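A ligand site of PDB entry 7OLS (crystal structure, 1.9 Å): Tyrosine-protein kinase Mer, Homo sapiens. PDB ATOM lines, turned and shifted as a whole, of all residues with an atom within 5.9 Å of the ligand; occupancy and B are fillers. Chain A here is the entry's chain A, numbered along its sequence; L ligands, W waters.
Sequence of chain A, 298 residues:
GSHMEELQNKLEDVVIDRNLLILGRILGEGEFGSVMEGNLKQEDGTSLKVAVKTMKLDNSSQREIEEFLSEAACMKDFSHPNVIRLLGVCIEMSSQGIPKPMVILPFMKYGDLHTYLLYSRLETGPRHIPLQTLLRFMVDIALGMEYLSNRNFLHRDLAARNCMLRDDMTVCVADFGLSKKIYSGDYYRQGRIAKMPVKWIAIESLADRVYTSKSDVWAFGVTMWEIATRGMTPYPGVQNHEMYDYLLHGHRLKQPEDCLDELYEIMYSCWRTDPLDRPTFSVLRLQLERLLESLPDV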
ATOM      1  N   LEU A  27     -21.936   7.615  24.088  1.00  0.00           N
ATOM      2  CA  LEU A  27     -23.021   7.331  25.046  1.00  0.00           C
ATOM      3  C   LEU A  27     -22.563   7.517  26.485  1.00  0.00           C
ATOM      4  O   LEU A  27     -23.257   8.115  27.293  1.00  0.00           O
ATOM      5  CB  LEU A  27     -23.543   5.904  24.857  1.00  0.00           C
ATOM      6  CG  LEU A  27     -24.149   5.593  23.491  1.00  0.00           C
ATOM      7  CD1 LEU A  27     -24.373   4.098  23.306  1.00  0.00           C
ATOM      8  CD2 LEU A  27     -25.456   6.354  23.280  1.00  0.00           C
ATOM      9  N   VAL A  35     -18.085   4.222  25.828  1.00  0.00           N
ATOM     10  CA  VAL A  35     -19.134   3.475  25.131  1.00  0.00           C
ATOM     11  C   VAL A  35     -19.707   4.382  24.038  1.00  0.00           C
ATOM     12  O   VAL A  35     -19.950   5.566  24.281  1.00  0.00           O
ATOM     13  CB  VAL A  35     -20.252   3.026  26.086  1.00  0.00           C
ATOM     14  CG1 VAL A  35     -21.287   2.165  25.366  1.00  0.00           C
ATOM     15  CG2 VAL A  35     -19.671   2.266  27.274  1.00  0.00           C
ATOM     16  N   ALA A  51     -23.401  -1.411  20.155  1.00  0.00           N
ATOM     17  CA  ALA A  51     -22.651  -0.644  21.144  1.00  0.00           C
ATOM     18  C   ALA A  51     -21.180  -0.987  20.981  1.00  0.00           C
ATOM     19  O   ALA A  51     -20.837  -2.153  20.834  1.00  0.00           O
ATOM     20  CB  ALA A  51     -23.116  -0.984  22.557  1.00  0.00           C
ATOM     21  N   LYS A  53     -17.514  -0.558  22.849  1.00  0.00           N
ATOM     22  CA  LYS A  53     -16.720  -0.210  24.045  1.00  0.00           C
ATOM     23  C   LYS A  53     -15.240  -0.141  23.675  1.00  0.00           C
ATOM     24  O   LYS A  53     -14.642  -1.150  23.301  1.00  0.00           O
ATOM     25  CB  LYS A  53     -16.956  -1.227  25.167  1.00  0.00           C
ATOM     26  CG  LYS A  53     -16.078  -1.083  26.403  1.00  0.00           C
ATOM     27  CD  LYS A  53     -16.099   0.316  27.006  1.00  0.00           C
ATOM     28  CE  LYS A  53     -15.204   0.429  28.232  1.00  0.00           C
ATOM     29  NZ  LYS A  53     -15.726  -0.325  29.396  1.00  0.00           N
ATOM     30  N   MET A  55     -11.360   0.581  24.840  1.00  0.00           N
ATOM     31  CA  MET A  55     -10.597   0.385  26.079  1.00  0.00           C
ATOM     32  C   MET A  55      -9.561   1.491  26.281  1.00  0.00           C
ATOM     33  O   MET A  55      -8.495   1.479  25.680  1.00  0.00           O
ATOM     34  CB  MET A  55      -9.914  -0.992  26.083  1.00  0.00           C
ATOM     35  CG  MET A  55     -10.844  -2.177  25.820  1.00  0.00           C
ATOM     36  SD  MET A  55     -12.082  -2.477  27.099  1.00  0.00           S
ATOM     37  CE  MET A  55     -11.050  -3.039  28.452  1.00  0.00           C
ATOM     38  N   GLU A  67      -3.168 -10.773  24.678  1.00  0.00           N
ATOM     39  CA  GLU A  67      -3.941 -11.214  25.842  1.00  0.00           C
ATOM     40  C   GLU A  67      -5.413 -10.790  25.740  1.00  0.00           C
ATOM     41  O   GLU A  67      -6.315 -11.539  26.116  1.00  0.00           O
ATOM     42  CB  GLU A  67      -3.301 -10.661  27.117  1.00  0.00           C
ATOM     43  CG  GLU A  67      -3.811 -11.264  28.416  1.00  0.00           C
ATOM     44  CD  GLU A  67      -2.950 -10.896  29.613  1.00  0.00           C
ATOM     45  OE1 GLU A  67      -2.218  -9.874  29.549  1.00  0.00           O
ATOM     46  OE2 GLU A  67      -2.999 -11.626  30.621  1.00  0.00           O
ATOM     47  N   PHE A  68      -5.634  -9.571  25.234  1.00  0.00           N
ATOM     48  CA  PHE A  68      -6.984  -9.052  24.965  1.00  0.00           C
ATOM     49  C   PHE A  68      -7.687  -9.858  23.860  1.00  0.00           C
ATOM     50  O   PHE A  68      -8.860 -10.208  24.002  1.00  0.00           O
ATOM     51  CB  PHE A  68      -6.903  -7.557  24.590  1.00  0.00           C
ATOM     52  CG  PHE A  68      -8.184  -6.995  24.046  1.00  0.00           C
ATOM     53  CD1 PHE A  68      -9.164  -6.514  24.908  1.00  0.00           C
ATOM     54  CD2 PHE A  68      -8.403  -6.934  22.677  1.00  0.00           C
ATOM     55  CE1 PHE A  68     -10.349  -5.987  24.406  1.00  0.00           C
ATOM     56  CE2 PHE A  68      -9.585  -6.420  22.168  1.00  0.00           C
ATOM     57  CZ  PHE A  68     -10.553  -5.945  23.032  1.00  0.00           C
ATOM     58  N   LEU A  69      -6.984 -10.127  22.770  1.00  0.00           N
ATOM     59  CA  LEU A  69      -7.529 -10.944  21.663  1.00  0.00           C
ATOM     60  C   LEU A  69      -7.815 -12.383  22.079  1.00  0.00           C
ATOM     61  O   LEU A  69      -8.818 -12.963  21.659  1.00  0.00           O
ATOM     62  CB  LEU A  69      -6.574 -10.938  20.462  1.00  0.00           C
ATOM     63  CG  LEU A  69      -6.419  -9.600  19.715  1.00  0.00           C
ATOM     64  CD1 LEU A  69      -5.146  -9.597  18.897  1.00  0.00           C
ATOM     65  CD2 LEU A  69      -7.639  -9.337  18.843  1.00  0.00           C
ATOM     66  N   GLU A  71      -8.424 -13.439  25.256  1.00  0.00           N
ATOM     67  CA  GLU A  71      -9.569 -13.329  26.166  1.00  0.00           C
ATOM     68  C   GLU A  71     -10.870 -13.065  25.391  1.00  0.00           C
ATOM     69  O   GLU A  71     -11.902 -13.661  25.683  1.00  0.00           O
ATOM     70  CB  GLU A  71      -9.306 -12.229  27.210  1.00  0.00           C
ATOM     71  CG  GLU A  71     -10.397 -12.010  28.259  1.00  0.00           C
ATOM     72  CD  GLU A  71     -10.547 -13.148  29.251  1.00  0.00           C
ATOM     73  OE1 GLU A  71     -10.129 -12.985  30.413  1.00  0.00           O
ATOM     74  OE2 GLU A  71     -11.075 -14.218  28.867  1.00  0.00           O
ATOM     75  N   ALA A  72     -10.805 -12.168  24.406  1.00  0.00           N
ATOM     76  CA  ALA A  72     -11.961 -11.857  23.556  1.00  0.00           C
ATOM     77  C   ALA A  72     -12.445 -13.090  22.804  1.00  0.00           C
ATOM     78  O   ALA A  72     -13.647 -13.317  22.699  1.00  0.00           O
ATOM     79  CB  ALA A  72     -11.628 -10.739  22.575  1.00  0.00           C
ATOM     80  N   MET A  75     -14.594 -15.252  25.137  1.00  0.00           N
ATOM     81  CA  MET A  75     -15.909 -14.642  25.398  1.00  0.00           C
ATOM     82  C   MET A  75     -16.852 -14.717  24.192  1.00  0.00           C
ATOM     83  O   MET A  75     -18.037 -14.965  24.350  1.00  0.00           O
ATOM     84  CB  MET A  75     -15.763 -13.192  25.859  1.00  0.00           C
ATOM     85  CG  MET A  75     -15.111 -13.031  27.226  1.00  0.00           C
ATOM     86  SD  MET A  75     -14.574 -11.349  27.532  1.00  0.00           S
ATOM     87  CE  MET A  75     -13.925 -11.488  29.202  1.00  0.00           C
ATOM     88  N   ILE A  84     -24.393 -11.882  27.685  1.00  0.00           N
ATOM     89  CA  ILE A  84     -24.240 -10.960  26.549  1.00  0.00           C
ATOM     90  C   ILE A  84     -23.323 -11.583  25.496  1.00  0.00           C
ATOM     91  O   ILE A  84     -22.298 -12.183  25.829  1.00  0.00           O
ATOM     92  CB  ILE A  84     -23.712  -9.564  26.983  1.00  0.00           C
ATOM     93  CG1 ILE A  84     -23.944  -8.532  25.874  1.00  0.00           C
ATOM     94  CG2 ILE A  84     -22.232  -9.605  27.379  1.00  0.00           C
ATOM     95  CD1 ILE A  84     -23.900  -7.106  26.379  1.00  0.00           C
ATOM     96  N   LEU A  86     -20.683 -11.346  22.652  1.00  0.00           N
ATOM     97  CA  LEU A  86     -19.677 -10.513  22.028  1.00  0.00           C
ATOM     98  C   LEU A  86     -19.760 -10.749  20.518  1.00  0.00           C
ATOM     99  O   LEU A  86     -19.627 -11.885  20.069  1.00  0.00           O
ATOM    100  CB  LEU A  86     -18.283 -10.905  22.557  1.00  0.00           C
ATOM    101  CG  LEU A  86     -17.058 -10.250  21.938  1.00  0.00           C
ATOM    102  CD1 LEU A  86     -17.124  -8.751  22.122  1.00  0.00           C
ATOM    103  CD2 LEU A  86     -15.798 -10.812  22.557  1.00  0.00           C
ATOM    104  N   VAL A  89     -14.279  -7.970  17.841  1.00  0.00           N
ATOM    105  CA  VAL A  89     -13.322  -6.943  18.257  1.00  0.00           C
ATOM    106  C   VAL A  89     -12.642  -6.269  17.053  1.00  0.00           C
ATOM    107  O   VAL A  89     -12.462  -6.881  16.003  1.00  0.00           O
ATOM    108  CB  VAL A  89     -12.246  -7.513  19.217  1.00  0.00           C
ATOM    109  CG1 VAL A  89     -12.892  -8.028  20.499  1.00  0.00           C
ATOM    110  CG2 VAL A  89     -11.420  -8.620  18.571  1.00  0.00           C
ATOM    111  N   VAL A 103     -14.496  -3.181  21.422  1.00  0.00           N
ATOM    112  CA  VAL A 103     -15.346  -4.342  21.681  1.00  0.00           C
ATOM    113  C   VAL A 103     -16.753  -4.009  21.184  1.00  0.00           C
ATOM    114  O   VAL A 103     -17.332  -3.010  21.605  1.00  0.00           O
ATOM    115  CB  VAL A 103     -15.399  -4.663  23.189  1.00  0.00           C
ATOM    116  CG1 VAL A 103     -16.237  -5.895  23.485  1.00  0.00           C
ATOM    117  CG2 VAL A 103     -13.996  -4.866  23.745  1.00  0.00           C
ATOM    118  N   LEU A 105     -20.744  -4.888  20.648  1.00  0.00           N
ATOM    119  CA  LEU A 105     -21.794  -5.551  21.413  1.00  0.00           C
ATOM    120  C   LEU A 105     -23.158  -5.231  20.813  1.00  0.00           C
ATOM    121  O   LEU A 105     -23.302  -4.195  20.168  1.00  0.00           O
ATOM    122  CB  LEU A 105     -21.761  -5.058  22.851  1.00  0.00           C
ATOM    123  CG  LEU A 105     -20.437  -5.265  23.582  1.00  0.00           C
ATOM    124  CD1 LEU A 105     -20.326  -4.320  24.775  1.00  0.00           C
ATOM    125  CD2 LEU A 105     -20.296  -6.708  24.015  1.00  0.00           C
ATOM    126  N   PRO A 106     -24.165  -6.096  21.043  1.00  0.00           N
ATOM    127  CA  PRO A 106     -25.527  -5.724  20.647  1.00  0.00           C
ATOM    128  C   PRO A 106     -25.988  -4.484  21.401  1.00  0.00           C
ATOM    129  O   PRO A 106     -25.744  -4.386  22.614  1.00  0.00           O
ATOM    130  CB  PRO A 106     -26.365  -6.939  21.054  1.00  0.00           C
ATOM    131  CG  PRO A 106     -25.402  -8.051  21.237  1.00  0.00           C
ATOM    132  CD  PRO A 106     -24.130  -7.415  21.690  1.00  0.00           C
ATOM    133  N   PHE A 107     -26.621  -3.554  20.696  1.00  0.00           N
ATOM    134  CA  PHE A 107     -27.159  -2.357  21.330  1.00  0.00           C
ATOM    135  C   PHE A 107     -28.394  -2.732  22.156  1.00  0.00           C
ATOM    136  O   PHE A 107     -29.283  -3.438  21.661  1.00  0.00           O
ATOM    137  CB  PHE A 107     -27.534  -1.294  20.300  1.00  0.00           C
ATOM    138  CG  PHE A 107     -27.850   0.040  20.896  1.00  0.00           C
ATOM    139  CD1 PHE A 107     -26.843   0.954  21.170  1.00  0.00           C
ATOM    140  CD2 PHE A 107     -29.164   0.375  21.216  1.00  0.00           C
ATOM    141  CE1 PHE A 107     -27.132   2.193  21.725  1.00  0.00           C
ATOM    142  CE2 PHE A 107     -29.460   1.606  21.785  1.00  0.00           C
ATOM    143  CZ  PHE A 107     -28.444   2.515  22.040  1.00  0.00           C
ATOM    144  N   MET A 108     -28.435  -2.252  23.399  1.00  0.00           N
ATOM    145  CA  MET A 108     -29.516  -2.565  24.335  1.00  0.00           C
ATOM    146  C   MET A 108     -30.117  -1.256  24.844  1.00  0.00           C
ATOM    147  O   MET A 108     -29.604  -0.644  25.803  1.00  0.00           O
ATOM    148  CB  MET A 108     -28.977  -3.431  25.478  1.00  0.00           C
ATOM    149  CG  MET A 108     -28.177  -4.615  24.979  1.00  0.00           C
ATOM    150  SD  MET A 108     -28.265  -6.066  26.031  1.00  0.00           S
ATOM    151  CE  MET A 108     -27.462  -7.289  24.992  1.00  0.00           C
ATOM    152  N   LYS A 109     -31.189  -0.811  24.176  1.00  0.00           N
ATOM    153  CA  LYS A 109     -31.771   0.503  24.437  1.00  0.00           C
ATOM    154  C   LYS A 109     -32.321   0.689  25.850  1.00  0.00           C
ATOM    155  O   LYS A 109     -32.340   1.807  26.344  1.00  0.00           O
ATOM    156  CB  LYS A 109     -32.815   0.877  23.367  1.00  0.00           C
ATOM    157  CG  LYS A 109     -34.078   0.028  23.323  1.00  0.00           C
ATOM    158  CD  LYS A 109     -34.972   0.470  22.170  1.00  0.00           C
ATOM    159  CE  LYS A 109     -35.967  -0.605  21.773  1.00  0.00           C
ATOM    160  NZ  LYS A 109     -36.892  -0.953  22.886  1.00  0.00           N
ATOM    161  N   GLY A 111     -30.842  -0.436  28.526  1.00  0.00           N
ATOM    162  CA  GLY A 111     -29.689  -0.133  29.373  1.00  0.00           C
ATOM    163  C   GLY A 111     -29.419  -1.162  30.459  1.00  0.00           C
ATOM    164  O   GLY A 111     -29.860  -2.314  30.358  1.00  0.00           O
ATOM    165  N   MET A 164     -27.523  -6.379  31.796  1.00  0.00           N
ATOM    166  CA  MET A 164     -28.147  -5.575  30.764  1.00  0.00           C
ATOM    167  C   MET A 164     -29.527  -6.134  30.425  1.00  0.00           C
ATOM    168  O   MET A 164     -29.730  -7.347  30.455  1.00  0.00           O
ATOM    169  CB  MET A 164     -27.266  -5.542  29.513  1.00  0.00           C
ATOM    170  CG  MET A 164     -25.897  -4.880  29.717  1.00  0.00           C
ATOM    171  SD  MET A 164     -25.920  -3.111  30.098  1.00  0.00           S
ATOM    172  CE  MET A 164     -26.763  -2.423  28.670  1.00  0.00           C
ATOM    173  N   ALA A 174     -23.082  -9.269  31.865  1.00  0.00           N
ATOM    174  CA  ALA A 174     -22.217  -8.514  30.955  1.00  0.00           C
ATOM    175  C   ALA A 174     -21.031  -7.888  31.692  1.00  0.00           C
ATOM    176  O   ALA A 174     -20.852  -8.134  32.886  1.00  0.00           O
ATOM    177  CB  ALA A 174     -23.040  -7.437  30.257  1.00  0.00           C
ATOM    178  N   ASP A 175     -20.234  -7.094  30.973  1.00  0.00           N
ATOM    179  CA  ASP A 175     -19.168  -6.260  31.563  1.00  0.00           C
ATOM    180  C   ASP A 175     -18.236  -7.080  32.460  1.00  0.00           C
ATOM    181  O   ASP A 175     -18.091  -6.797  33.652  1.00  0.00           O
ATOM    182  CB  ASP A 175     -19.767  -5.047  32.321  1.00  0.00           C
ATOM    183  CG  ASP A 175     -19.610  -3.725  31.559  1.00  0.00           C
ATOM    184  OD1 ASP A 175     -18.554  -3.498  30.923  1.00  0.00           O
ATOM    185  OD2 ASP A 175     -20.535  -2.893  31.638  1.00  0.00           O
ATOM    186  N   PHE A 176     -17.612  -8.092  31.873  1.00  0.00           N
ATOM    187  CA  PHE A 176     -16.853  -9.089  32.629  1.00  0.00           C
ATOM    188  C   PHE A 176     -15.546  -8.477  33.143  1.00  0.00           C
ATOM    189  O   PHE A 176     -14.917  -7.668  32.446  1.00  0.00           O
ATOM    190  CB  PHE A 176     -16.552 -10.323  31.773  1.00  0.00           C
ATOM    191  CG  PHE A 176     -17.770 -10.909  31.108  1.00  0.00           C
ATOM    192  CD1 PHE A 176     -18.742 -11.553  31.863  1.00  0.00           C
ATOM    193  CD2 PHE A 176     -17.958 -10.811  29.723  1.00  0.00           C
ATOM    194  CE1 PHE A 176     -19.871 -12.091  31.262  1.00  0.00           C
ATOM    195  CE2 PHE A 176     -19.086 -11.349  29.122  1.00  0.00           C
ATOM    196  CZ  PHE A 176     -20.047 -11.996  29.889  1.00  0.00           C
HETATM  197  C1  LIG L   1     -22.413  -2.220  28.632  1.00  0.00           C
HETATM  198  C2  LIG L   1     -23.393  -1.918  27.523  1.00  0.00           C
HETATM  199  C3  LIG L   1     -23.772  -2.982  26.608  1.00  0.00           C
HETATM  200  N1  LIG L   1     -11.998  -8.353  26.784  1.00  0.00           N
HETATM  201  C4  LIG L   1     -25.499   0.678  25.948  1.00  0.00           C
HETATM  202  C5  LIG L   1     -23.936  -0.695  27.347  1.00  0.00           C
HETATM  203  C6  LIG L   1     -20.669  -3.823  28.082  1.00  0.00           C
HETATM  204  C7  LIG L   1     -19.192  -5.339  27.958  1.00  0.00           C
HETATM  205  C8  LIG L   1     -17.844  -5.905  27.796  1.00  0.00           C
HETATM  206  C9  LIG L   1     -16.760  -5.055  27.985  1.00  0.00           C
HETATM  207  C10 LIG L   1     -15.462  -5.521  27.862  1.00  0.00           C
HETATM  208  C11 LIG L   1     -15.224  -6.853  27.547  1.00  0.00           C
HETATM  209  C12 LIG L   1     -16.315  -7.711  27.372  1.00  0.00           C
HETATM  210  C13 LIG L   1     -17.630  -7.263  27.490  1.00  0.00           C
HETATM  211  C14 LIG L   1     -12.810  -7.203  28.363  1.00  0.00           C
HETATM  212  C15 LIG L   1     -10.970  -9.088  26.068  1.00  0.00           C
HETATM  213  C16 LIG L   1     -13.281  -8.124  26.418  1.00  0.00           C
HETATM  214  C17 LIG L   1     -13.858  -8.636  25.146  1.00  0.00           C
HETATM  215  N2  LIG L   1     -11.691  -7.791  27.984  1.00  0.00           N
HETATM  216  C18 LIG L   1     -13.841  -7.370  27.429  1.00  0.00           C
HETATM  217  C19 LIG L   1     -18.747  -8.254  27.270  1.00  0.00           C
HETATM  218  O1  LIG L   1     -19.345  -3.986  27.836  1.00  0.00           O
HETATM  219  N3  LIG L   1     -20.294  -5.936  28.274  1.00  0.00           N
HETATM  220  N4  LIG L   1     -21.281  -4.940  28.338  1.00  0.00           N
HETATM  221  N5  LIG L   1     -21.142  -2.572  28.021  1.00  0.00           N
HETATM  222  C20 LIG L   1     -20.372  -1.480  27.417  1.00  0.00           C
HETATM  223  N6  LIG L   1     -24.825  -0.472  26.316  1.00  0.00           N
HETATM  224  C21 LIG L   1     -26.239   0.341  24.863  1.00  0.00           C
HETATM  225  N7  LIG L   1     -26.068  -0.986  24.526  1.00  0.00           N
HETATM  226  C22 LIG L   1     -25.196  -1.472  25.420  1.00  0.00           C
HETATM  227  C23 LIG L   1     -24.638  -2.760  25.588  1.00  0.00           C
HETATM  228  O   HOH W   1     -26.149   1.367  29.239  1.00  0.00           O
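N of Met 108 lies within hydrogen-bond range of N7 of the ligand (2.9 Å). A nitrogen (N3) of the ligand is in hydrogen-bond range of the backbone NH of Asp 175 (2.9 Å).
The backbone carbonyl oxygen of Ala 51 is in hydrogen-bond range of the backbone NH of Leu 105. The backbone NH (N) of Leu 27 is in hydrogen-bond range of the backbone carbonyl oxygen (O) of Val 35 (2.9 Å). The backbone carbonyl oxygen (O) of Val 103 is in hydrogen-bond range of the backbone NH (N) of Lys 53 (2.8 Å).
Val 35 touches the ligand. CB of Ala 51 touches N7 of the ligand, 3.5 Å away. O of Phe 68 touches C15 of the ligand, 3.2 Å away. CG of Glu 71 touches C15 of the ligand, at 3.7 Å. N of Ala 72 touches C15 of the ligand (3.5 Å). Met 75 touches the ligand (SD to C16, 3.6 Å). Ile 84 touches the ligand (CG2 to C19, 3.7 Å). Leu 86 touches the ligand (CD2 to C17, 3.9 Å). Val 103 touches the ligand (CG1 to C17, 3.99 Å). Leu 105 touches the ligand. O of Pro 106 touches C23 of the ligand (3.6 Å). Phe 107 touches the ligand. Met 164 touches the ligand (CE to C5, 3.6 Å). CB of Ala 174 touches N4 of the ligand, at 3.6 Å. Phe 176 touches the ligand (CE2 to C19, 3.6 Å). Hydrophobic or aromatic side chains that line the ligand: Val 35, Ala 51, Phe 68, Ala 72, Met 75, Ile 84, Leu 86, Val 103, Leu 105, Phe 107, Met 108, Met 164, Ala 174 and Phe 176. Within 4 Å of the ligand: Val 35, Ala 51, Phe 68, Glu 71, Ala 72, Met 75, Ile 84, Leu 86, Val 103, Leu 105, Pro 106, Phe 107, Met 108, Met 164, Ala 174, Asp 175 and Phe 176. The nearest printed residue that does not touch the ligand is Lys 53 (4.1 Å).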
